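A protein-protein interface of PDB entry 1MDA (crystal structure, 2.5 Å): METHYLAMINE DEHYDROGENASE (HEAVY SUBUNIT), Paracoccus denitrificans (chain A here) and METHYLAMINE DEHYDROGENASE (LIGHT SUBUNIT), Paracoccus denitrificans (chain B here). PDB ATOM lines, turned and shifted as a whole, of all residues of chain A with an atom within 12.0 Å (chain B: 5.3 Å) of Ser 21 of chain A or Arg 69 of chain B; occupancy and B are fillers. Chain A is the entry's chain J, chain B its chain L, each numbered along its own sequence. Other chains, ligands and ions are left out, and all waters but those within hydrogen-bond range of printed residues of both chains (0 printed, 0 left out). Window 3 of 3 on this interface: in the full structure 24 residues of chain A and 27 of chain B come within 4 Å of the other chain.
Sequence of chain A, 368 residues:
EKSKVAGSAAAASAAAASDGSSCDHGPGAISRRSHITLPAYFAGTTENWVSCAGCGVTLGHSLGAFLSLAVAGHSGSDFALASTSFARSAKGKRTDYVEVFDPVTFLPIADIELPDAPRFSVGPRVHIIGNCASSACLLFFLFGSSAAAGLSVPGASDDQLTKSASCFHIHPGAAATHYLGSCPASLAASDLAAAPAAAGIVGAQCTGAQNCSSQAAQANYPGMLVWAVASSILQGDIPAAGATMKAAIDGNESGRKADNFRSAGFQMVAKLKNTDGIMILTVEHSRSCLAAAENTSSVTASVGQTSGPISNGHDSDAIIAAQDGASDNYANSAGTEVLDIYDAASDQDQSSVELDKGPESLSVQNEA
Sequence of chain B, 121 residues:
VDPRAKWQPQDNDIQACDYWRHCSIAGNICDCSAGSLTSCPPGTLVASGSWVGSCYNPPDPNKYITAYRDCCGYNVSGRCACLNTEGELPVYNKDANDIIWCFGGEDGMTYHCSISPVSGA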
ATOM      1  N   ALA A   9     -32.607  -5.593  -0.453  1.00  0.00           N
ATOM      2  CA  ALA A   9     -32.860  -6.320  -1.672  1.00  0.00           C
ATOM      3  C   ALA A   9     -33.726  -5.523  -2.616  1.00  0.00           C
ATOM      4  O   ALA A   9     -33.552  -5.620  -3.823  1.00  0.00           O
ATOM      5  CB  ALA A   9     -33.428  -7.713  -1.452  1.00  0.00           C
ATOM      6  N   ALA A  12     -31.396  -3.619  -4.430  1.00  0.00           N
ATOM      7  CA  ALA A  12     -30.636  -4.367  -5.423  1.00  0.00           C
ATOM      8  C   ALA A  12     -31.471  -4.678  -6.659  1.00  0.00           C
ATOM      9  O   ALA A  12     -31.002  -4.549  -7.806  1.00  0.00           O
ATOM     10  CB  ALA A  12     -30.039  -5.666  -4.849  1.00  0.00           C
ATOM     11  N   ALA A  17     -29.627  -5.970 -10.092  1.00  0.00           N
ATOM     12  CA  ALA A  17     -28.559  -6.848  -9.674  1.00  0.00           C
ATOM     13  C   ALA A  17     -28.855  -8.269  -9.185  1.00  0.00           C
ATOM     14  O   ALA A  17     -29.703  -8.553  -8.348  1.00  0.00           O
ATOM     15  CB  ALA A  17     -27.600  -6.137  -8.723  1.00  0.00           C
ATOM     16  N   SER A  18     -28.112  -9.146  -9.808  1.00  0.00           N
ATOM     17  CA  SER A  18     -27.707 -10.485  -9.481  1.00  0.00           C
ATOM     18  C   SER A  18     -28.543 -11.623  -8.910  1.00  0.00           C
ATOM     19  O   SER A  18     -28.957 -12.554  -9.603  1.00  0.00           O
ATOM     20  CB  SER A  18     -26.645 -10.191  -8.422  1.00  0.00           C
ATOM     21  OG  SER A  18     -26.081 -11.356  -7.852  1.00  0.00           O
ATOM     22  N   ASP A  19     -28.570 -11.643  -7.579  1.00  0.00           N
ATOM     23  CA  ASP A  19     -29.042 -12.793  -6.824  1.00  0.00           C
ATOM     24  C   ASP A  19     -28.213 -14.023  -7.263  1.00  0.00           C
ATOM     25  O   ASP A  19     -28.662 -14.858  -8.059  1.00  0.00           O
ATOM     26  CB  ASP A  19     -30.562 -13.043  -6.732  1.00  0.00           C
ATOM     27  CG  ASP A  19     -31.300 -12.109  -5.823  1.00  0.00           C
ATOM     28  OD1 ASP A  19     -30.515 -11.208  -5.253  1.00  0.00           O
ATOM     29  OD2 ASP A  19     -32.504 -12.215  -5.624  1.00  0.00           O
ATOM     30  N   GLY A  20     -26.929 -14.001  -6.847  1.00  0.00           N
ATOM     31  CA  GLY A  20     -25.923 -15.025  -7.084  1.00  0.00           C
ATOM     32  C   GLY A  20     -25.593 -15.689  -5.764  1.00  0.00           C
ATOM     33  O   GLY A  20     -24.744 -15.220  -5.005  1.00  0.00           O
ATOM     34  N   SER A  21     -26.252 -16.812  -5.540  1.00  0.00           N
ATOM     35  CA  SER A  21     -26.171 -17.520  -4.283  1.00  0.00           C
ATOM     36  C   SER A  21     -24.846 -18.238  -4.025  1.00  0.00           C
ATOM     37  O   SER A  21     -24.256 -18.833  -4.935  1.00  0.00           O
ATOM     38  CB  SER A  21     -27.376 -18.409  -4.257  1.00  0.00           C
ATOM     39  OG  SER A  21     -28.338 -17.731  -5.065  1.00  0.00           O
ATOM     40  N   SER A  22     -24.436 -18.200  -2.750  1.00  0.00           N
ATOM     41  CA  SER A  22     -23.226 -18.809  -2.209  1.00  0.00           C
ATOM     42  C   SER A  22     -23.377 -19.062  -0.695  1.00  0.00           C
ATOM     43  O   SER A  22     -24.377 -18.662  -0.099  1.00  0.00           O
ATOM     44  CB  SER A  22     -21.976 -17.960  -2.453  1.00  0.00           C
ATOM     45  OG  SER A  22     -21.980 -16.749  -1.696  1.00  0.00           O
ATOM     46  N   CYS A  23     -22.450 -19.845  -0.118  1.00  0.00           N
ATOM     47  CA  CYS A  23     -22.462 -20.150   1.308  1.00  0.00           C
ATOM     48  C   CYS A  23     -21.697 -19.035   1.956  1.00  0.00           C
ATOM     49  O   CYS A  23     -20.588 -18.731   1.538  1.00  0.00           O
ATOM     50  CB  CYS A  23     -21.712 -21.439   1.669  1.00  0.00           C
ATOM     51  SG  CYS A  23     -21.925 -22.810   0.481  1.00  0.00           S
ATOM     52  N   ASP A  24     -22.275 -18.355   2.910  1.00  0.00           N
ATOM     53  CA  ASP A  24     -21.519 -17.283   3.501  1.00  0.00           C
ATOM     54  C   ASP A  24     -20.645 -17.655   4.676  1.00  0.00           C
ATOM     55  O   ASP A  24     -20.611 -18.817   5.056  1.00  0.00           O
ATOM     56  CB  ASP A  24     -22.173 -15.899   3.501  1.00  0.00           C
ATOM     57  CG  ASP A  24     -23.564 -15.885   4.008  1.00  0.00           C
ATOM     58  OD1 ASP A  24     -23.994 -16.736   4.746  1.00  0.00           O
ATOM     59  OD2 ASP A  24     -24.271 -14.900   3.478  1.00  0.00           O
ATOM     60  N   HIS A  25     -19.935 -16.667   5.259  1.00  0.00           N
ATOM     61  CA  HIS A  25     -19.086 -16.902   6.427  1.00  0.00           C
ATOM     62  C   HIS A  25     -19.232 -16.006   7.653  1.00  0.00           C
ATOM     63  O   HIS A  25     -19.394 -14.790   7.530  1.00  0.00           O
ATOM     64  CB  HIS A  25     -17.768 -17.730   6.381  1.00  0.00           C
ATOM     65  CG  HIS A  25     -16.575 -17.275   5.600  1.00  0.00           C
ATOM     66  ND1 HIS A  25     -15.901 -16.094   5.873  1.00  0.00           N
ATOM     67  CD2 HIS A  25     -15.784 -18.005   4.752  1.00  0.00           C
ATOM     68  CE1 HIS A  25     -14.829 -16.065   5.074  1.00  0.00           C
ATOM     69  NE2 HIS A  25     -14.711 -17.212   4.407  1.00  0.00           N
ATOM     70  N   THR B  38     -30.593 -14.713   0.168  1.00  0.00           N
ATOM     71  CA  THR B  38     -30.200 -15.481  -0.992  1.00  0.00           C
ATOM     72  C   THR B  38     -28.903 -16.215  -0.793  1.00  0.00           C
ATOM     73  O   THR B  38     -28.398 -16.871  -1.714  1.00  0.00           O
ATOM     74  CB  THR B  38     -30.066 -14.599  -2.229  1.00  0.00           C
ATOM     75  OG1 THR B  38     -29.121 -13.603  -1.930  1.00  0.00           O
ATOM     76  CG2 THR B  38     -31.414 -13.985  -2.565  1.00  0.00           C
ATOM     77  N   SER B  39     -28.447 -16.212   0.450  1.00  0.00           N
ATOM     78  CA  SER B  39     -27.227 -16.897   0.807  1.00  0.00           C
ATOM     79  C   SER B  39     -27.444 -17.800   2.025  1.00  0.00           C
ATOM     80  O   SER B  39     -28.328 -17.555   2.848  1.00  0.00           O
ATOM     81  CB  SER B  39     -26.106 -15.931   1.035  1.00  0.00           C
ATOM     82  OG  SER B  39     -25.882 -15.114  -0.119  1.00  0.00           O
ATOM     83  N   VAL B  46     -25.212 -25.671  -0.162  1.00  0.00           N
ATOM     84  CA  VAL B  46     -26.196 -25.176  -1.132  1.00  0.00           C
ATOM     85  C   VAL B  46     -26.509 -26.207  -2.213  1.00  0.00           C
ATOM     86  O   VAL B  46     -25.622 -26.773  -2.861  1.00  0.00           O
ATOM     87  CB  VAL B  46     -25.617 -23.904  -1.779  1.00  0.00           C
ATOM     88  CG1 VAL B  46     -26.654 -22.973  -2.401  1.00  0.00           C
ATOM     89  CG2 VAL B  46     -24.775 -23.149  -0.766  1.00  0.00           C
ATOM     90  N   ALA B  47     -27.785 -26.429  -2.432  1.00  0.00           N
ATOM     91  CA  ALA B  47     -28.236 -27.362  -3.443  1.00  0.00           C
ATOM     92  C   ALA B  47     -28.209 -26.729  -4.809  1.00  0.00           C
ATOM     93  O   ALA B  47     -27.980 -25.530  -4.911  1.00  0.00           O
ATOM     94  CB  ALA B  47     -29.670 -27.764  -3.167  1.00  0.00           C
ATOM     95  N   SER B  48     -28.410 -27.591  -5.814  1.00  0.00           N
ATOM     96  CA  SER B  48     -28.600 -27.282  -7.218  1.00  0.00           C
ATOM     97  C   SER B  48     -30.078 -27.349  -7.537  1.00  0.00           C
ATOM     98  O   SER B  48     -30.648 -26.506  -8.227  1.00  0.00           O
ATOM     99  CB  SER B  48     -27.830 -28.190  -8.179  1.00  0.00           C
ATOM    100  OG  SER B  48     -26.589 -27.573  -8.478  1.00  0.00           O
ATOM    101  N   GLY B  49     -30.686 -28.394  -6.997  1.00  0.00           N
ATOM    102  CA  GLY B  49     -32.099 -28.581  -7.153  1.00  0.00           C
ATOM    103  C   GLY B  49     -32.864 -27.424  -6.516  1.00  0.00           C
ATOM    104  O   GLY B  49     -32.425 -26.737  -5.584  1.00  0.00           O
ATOM    105  N   SER B  50     -34.051 -27.218  -7.036  1.00  0.00           N
ATOM    106  CA  SER B  50     -34.908 -26.198  -6.508  1.00  0.00           C
ATOM    107  C   SER B  50     -36.286 -26.376  -7.070  1.00  0.00           C
ATOM    108  O   SER B  50     -36.548 -27.193  -7.953  1.00  0.00           O
ATOM    109  CB  SER B  50     -34.409 -24.808  -6.833  1.00  0.00           C
ATOM    110  OG  SER B  50     -34.464 -24.615  -8.235  1.00  0.00           O
ATOM    111  N   ALA B  67     -36.475 -19.133  -7.313  1.00  0.00           N
ATOM    112  CA  ALA B  67     -35.951 -20.496  -7.253  1.00  0.00           C
ATOM    113  C   ALA B  67     -35.592 -20.897  -5.834  1.00  0.00           C
ATOM    114  O   ALA B  67     -34.484 -20.605  -5.392  1.00  0.00           O
ATOM    115  CB  ALA B  67     -34.765 -20.709  -8.163  1.00  0.00           C
ATOM    116  N   TYR B  68     -36.503 -21.609  -5.152  1.00  0.00           N
ATOM    117  CA  TYR B  68     -36.302 -21.988  -3.757  1.00  0.00           C
ATOM    118  C   TYR B  68     -35.304 -23.092  -3.567  1.00  0.00           C
ATOM    119  O   TYR B  68     -35.692 -24.269  -3.599  1.00  0.00           O
ATOM    120  CB  TYR B  68     -37.620 -22.364  -3.050  1.00  0.00           C
ATOM    121  CG  TYR B  68     -38.658 -21.269  -3.123  1.00  0.00           C
ATOM    122  CD1 TYR B  68     -38.618 -20.179  -2.250  1.00  0.00           C
ATOM    123  CD2 TYR B  68     -39.686 -21.335  -4.062  1.00  0.00           C
ATOM    124  CE1 TYR B  68     -39.556 -19.150  -2.336  1.00  0.00           C
ATOM    125  CE2 TYR B  68     -40.658 -20.344  -4.120  1.00  0.00           C
ATOM    126  CZ  TYR B  68     -40.583 -19.239  -3.273  1.00  0.00           C
ATOM    127  OH  TYR B  68     -41.520 -18.236  -3.373  1.00  0.00           O
ATOM    128  N   ARG B  69     -34.047 -22.693  -3.334  1.00  0.00           N
ATOM    129  CA  ARG B  69     -32.954 -23.629  -3.057  1.00  0.00           C
ATOM    130  C   ARG B  69     -32.753 -23.901  -1.587  1.00  0.00           C
ATOM    131  O   ARG B  69     -32.843 -22.990  -0.758  1.00  0.00           O
ATOM    132  CB  ARG B  69     -31.612 -23.327  -3.717  1.00  0.00           C
ATOM    133  CG  ARG B  69     -31.484 -23.947  -5.098  1.00  0.00           C
ATOM    134  CD  ARG B  69     -30.102 -23.745  -5.702  1.00  0.00           C
ATOM    135  NE  ARG B  69     -29.860 -22.376  -6.152  1.00  0.00           N
ATOM    136  CZ  ARG B  69     -28.660 -21.952  -6.550  1.00  0.00           C
ATOM    137  NH1 ARG B  69     -27.616 -22.781  -6.484  1.00  0.00           N
ATOM    138  NH2 ARG B  69     -28.474 -20.715  -6.965  1.00  0.00           N
ATOM    139  N   ASP B  70     -32.505 -25.165  -1.259  1.00  0.00           N
ATOM    140  CA  ASP B  70     -32.235 -25.486   0.108  1.00  0.00           C
ATOM    141  C   ASP B  70     -30.737 -25.442   0.412  1.00  0.00           C
ATOM    142  O   ASP B  70     -29.898 -25.646  -0.460  1.00  0.00           O
ATOM    143  CB  ASP B  70     -32.802 -26.859   0.525  1.00  0.00           C
ATOM    144  CG  ASP B  70     -34.283 -26.971   0.399  1.00  0.00           C
ATOM    145  OD1 ASP B  70     -34.849 -25.823   0.119  1.00  0.00           O
ATOM    146  OD2 ASP B  70     -34.884 -28.022   0.557  1.00  0.00           O
ATOM    147  N   CYS B  71     -30.419 -25.129   1.660  1.00  0.00           N
ATOM    148  CA  CYS B  71     -29.079 -25.207   2.207  1.00  0.00           C
ATOM    149  C   CYS B  71     -29.146 -26.464   3.036  1.00  0.00           C
ATOM    150  O   CYS B  71     -30.043 -26.589   3.874  1.00  0.00           O
ATOM    151  CB  CYS B  71     -28.829 -24.027   3.113  1.00  0.00           C
ATOM    152  SG  CYS B  71     -29.160 -22.473   2.279  1.00  0.00           S
ATOM    153  N   TRP B 101     -35.542 -30.351  -1.700  1.00  0.00           N
ATOM    154  CA  TRP B 101     -34.684 -29.996  -2.785  1.00  0.00           C
ATOM    155  C   TRP B 101     -33.276 -29.783  -2.257  1.00  0.00           C
ATOM    156  O   TRP B 101     -32.907 -28.659  -1.935  1.00  0.00           O
ATOM    157  CB  TRP B 101     -35.263 -28.690  -3.394  1.00  0.00           C
ATOM    158  CG  TRP B 101     -36.584 -28.913  -4.084  1.00  0.00           C
ATOM    159  CD1 TRP B 101     -37.721 -28.186  -4.072  1.00  0.00           C
ATOM    160  CD2 TRP B 101     -36.772 -29.762  -5.202  1.00  0.00           C
ATOM    161  NE1 TRP B 101     -38.650 -28.656  -4.885  1.00  0.00           N
ATOM    162  CE2 TRP B 101     -38.083 -29.596  -5.646  1.00  0.00           C
ATOM    163  CE3 TRP B 101     -35.979 -30.679  -5.841  1.00  0.00           C
ATOM    164  CZ2 TRP B 101     -38.610 -30.281  -6.709  1.00  0.00           C
ATOM    165  CZ3 TRP B 101     -36.510 -31.398  -6.872  1.00  0.00           C
ATOM    166  CH2 TRP B 101     -37.819 -31.239  -7.259  1.00  0.00           C
ATOM    167  N   CYS B 113     -32.528 -25.289   5.704  1.00  0.00           N
ATOM    168  CA  CYS B 113     -32.858 -23.992   5.231  1.00  0.00           C
ATOM    169  C   CYS B 113     -33.391 -23.887   3.806  1.00  0.00           C
ATOM    170  O   CYS B 113     -32.997 -24.634   2.912  1.00  0.00           O
ATOM    171  CB  CYS B 113     -31.439 -23.353   5.273  1.00  0.00           C
ATOM    172  SG  CYS B 113     -31.855 -21.767   5.892  1.00  0.00           S
ATOM    173  N   SER B 114     -34.119 -22.791   3.574  1.00  0.00           N
ATOM    174  CA  SER B 114     -34.700 -22.448   2.290  1.00  0.00           C
ATOM    175  C   SER B 114     -34.366 -21.023   1.937  1.00  0.00           C
ATOM    176  O   SER B 114     -34.631 -20.077   2.694  1.00  0.00           O
ATOM    177  CB  SER B 114     -36.199 -22.676   2.251  1.00  0.00           C
ATOM    178  OG  SER B 114     -36.465 -24.062   2.298  1.00  0.00           O
ATOM    179  N   ILE B 115     -33.708 -20.917   0.788  1.00  0.00           N
ATOM    180  CA  ILE B 115     -33.255 -19.638   0.246  1.00  0.00           C
ATOM    181  C   ILE B 115     -34.305 -19.100  -0.748  1.00  0.00           C
ATOM    182  O   ILE B 115     -35.029 -19.883  -1.387  1.00  0.00           O
ATOM    183  CB  ILE B 115     -31.878 -19.858  -0.357  1.00  0.00           C
ATOM    184  CG1 ILE B 115     -30.893 -18.802   0.106  1.00  0.00           C
ATOM    185  CG2 ILE B 115     -31.943 -19.808  -1.867  1.00  0.00           C
ATOM    186  CD1 ILE B 115     -29.503 -19.097  -0.451  1.00  0.00           C
ATOM    187  N   PRO B 117     -33.923 -16.714  -3.730  1.00  0.00           N
ATOM    188  CA  PRO B 117     -33.364 -15.920  -4.820  1.00  0.00           C
ATOM    189  C   PRO B 117     -34.271 -15.736  -6.038  1.00  0.00           C
ATOM    190  O   PRO B 117     -34.918 -16.661  -6.512  1.00  0.00           O
ATOM    191  CB  PRO B 117     -32.224 -16.763  -5.381  1.00  0.00           C
ATOM    192  CG  PRO B 117     -32.529 -18.198  -5.012  1.00  0.00           C
ATOM    193  CD  PRO B 117     -33.485 -18.132  -3.823  1.00  0.00           C
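Of the 11 printed residues of chain A, 5 touch a printed residue of chain B.
Among the printed residues, 7 pairs touch across the chains.
Among the printed residues, pairs that only touch across the chains: Cys 23 of chain A with Val 46 of chain B (3.1 Å), Asp 24 of chain A with Ser 39 of chain B (3.2 Å), Ser 22 of chain A with Ser 39 of chain B (3.4 Å), Ser 21 of chain A with Arg 69 of chain B (3.5 Å), Asp 19 of chain A with Thr 38 of chain B (3.7 Å) and Asp 19 of chain A with Pro 117 of chain B (3.9 Å).
The side-chain hydroxyl (OG) of Ser 21 of chain A lies close to the backbone carbonyl oxygen (O) of Thr 38 of chain B (3.5 Å).
O of Ala 47 of chain B lies close to NH1 of Arg 69 of chain B, 3.2 Å away.
The backbone carbonyl oxygen (O) of Pro 117 of chain B sits at hydrogen-bond distance from the backbone NH (N) of Ala 67 of chain B, at 3.0 Å.
The backbone carbonyl oxygen (O) of Arg 69 of chain B is in hydrogen-bond range of the backbone NH (N) of Ile 115 of chain B (2.7 Å).
Printed residues of chain B within 4 Å of Ser 21 of chain A: Thr 38 (3.1 Å) and Arg 69 (3.5 Å).
Of chain A, only Ser 22 (3.4 Å) and Asp 24 (3.2 Å) come within 4 Å of Ser 39 of chain B.
No residue of chain A comes within 4 Å of Ala 47 of chain B.
No residue of chain A comes within 4 Å of Ser 48 of chain B.
No residue of chain A comes within 4 Å of Gly 49 of chain B.
Ser 50 of chain B touches none of the printed residues of chain A.
No residue of chain A comes within 4 Å of Ala 67 of chain B.
No residue of chain A comes within 4 Å of Asp 70 of chain B.
No residue of chain A comes within 4 Å of Cys 71 of chain B.
No residue of chain A comes within 4 Å of Cys 113 of chain B.
No residue of chain A comes within 4 Å of Ile 115 of chain B.
Of the printed residues of chain B, Ser 22 of chain A touches Ser 39.
Of the printed residues of chain A, Pro 117 of chain B touches Asp 19.
Of the printed residues of chain B, Asp 24 of chain A touches Ser 39.
Ser 18 of chain A touches none of the printed residues of chain B.
The nearest printed residue of chain B that does not touch Ser 21 of chain A is Pro 117 of chain B (4.02 Å).
The nearest residue of chain A that does not touch Arg 69 of chain B is Gly 20 of chain A (5.9 Å).
The nearest printed residue of chain B that does not touch Asp 24 of chain A is Thr 38 of chain B (6.4 Å).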
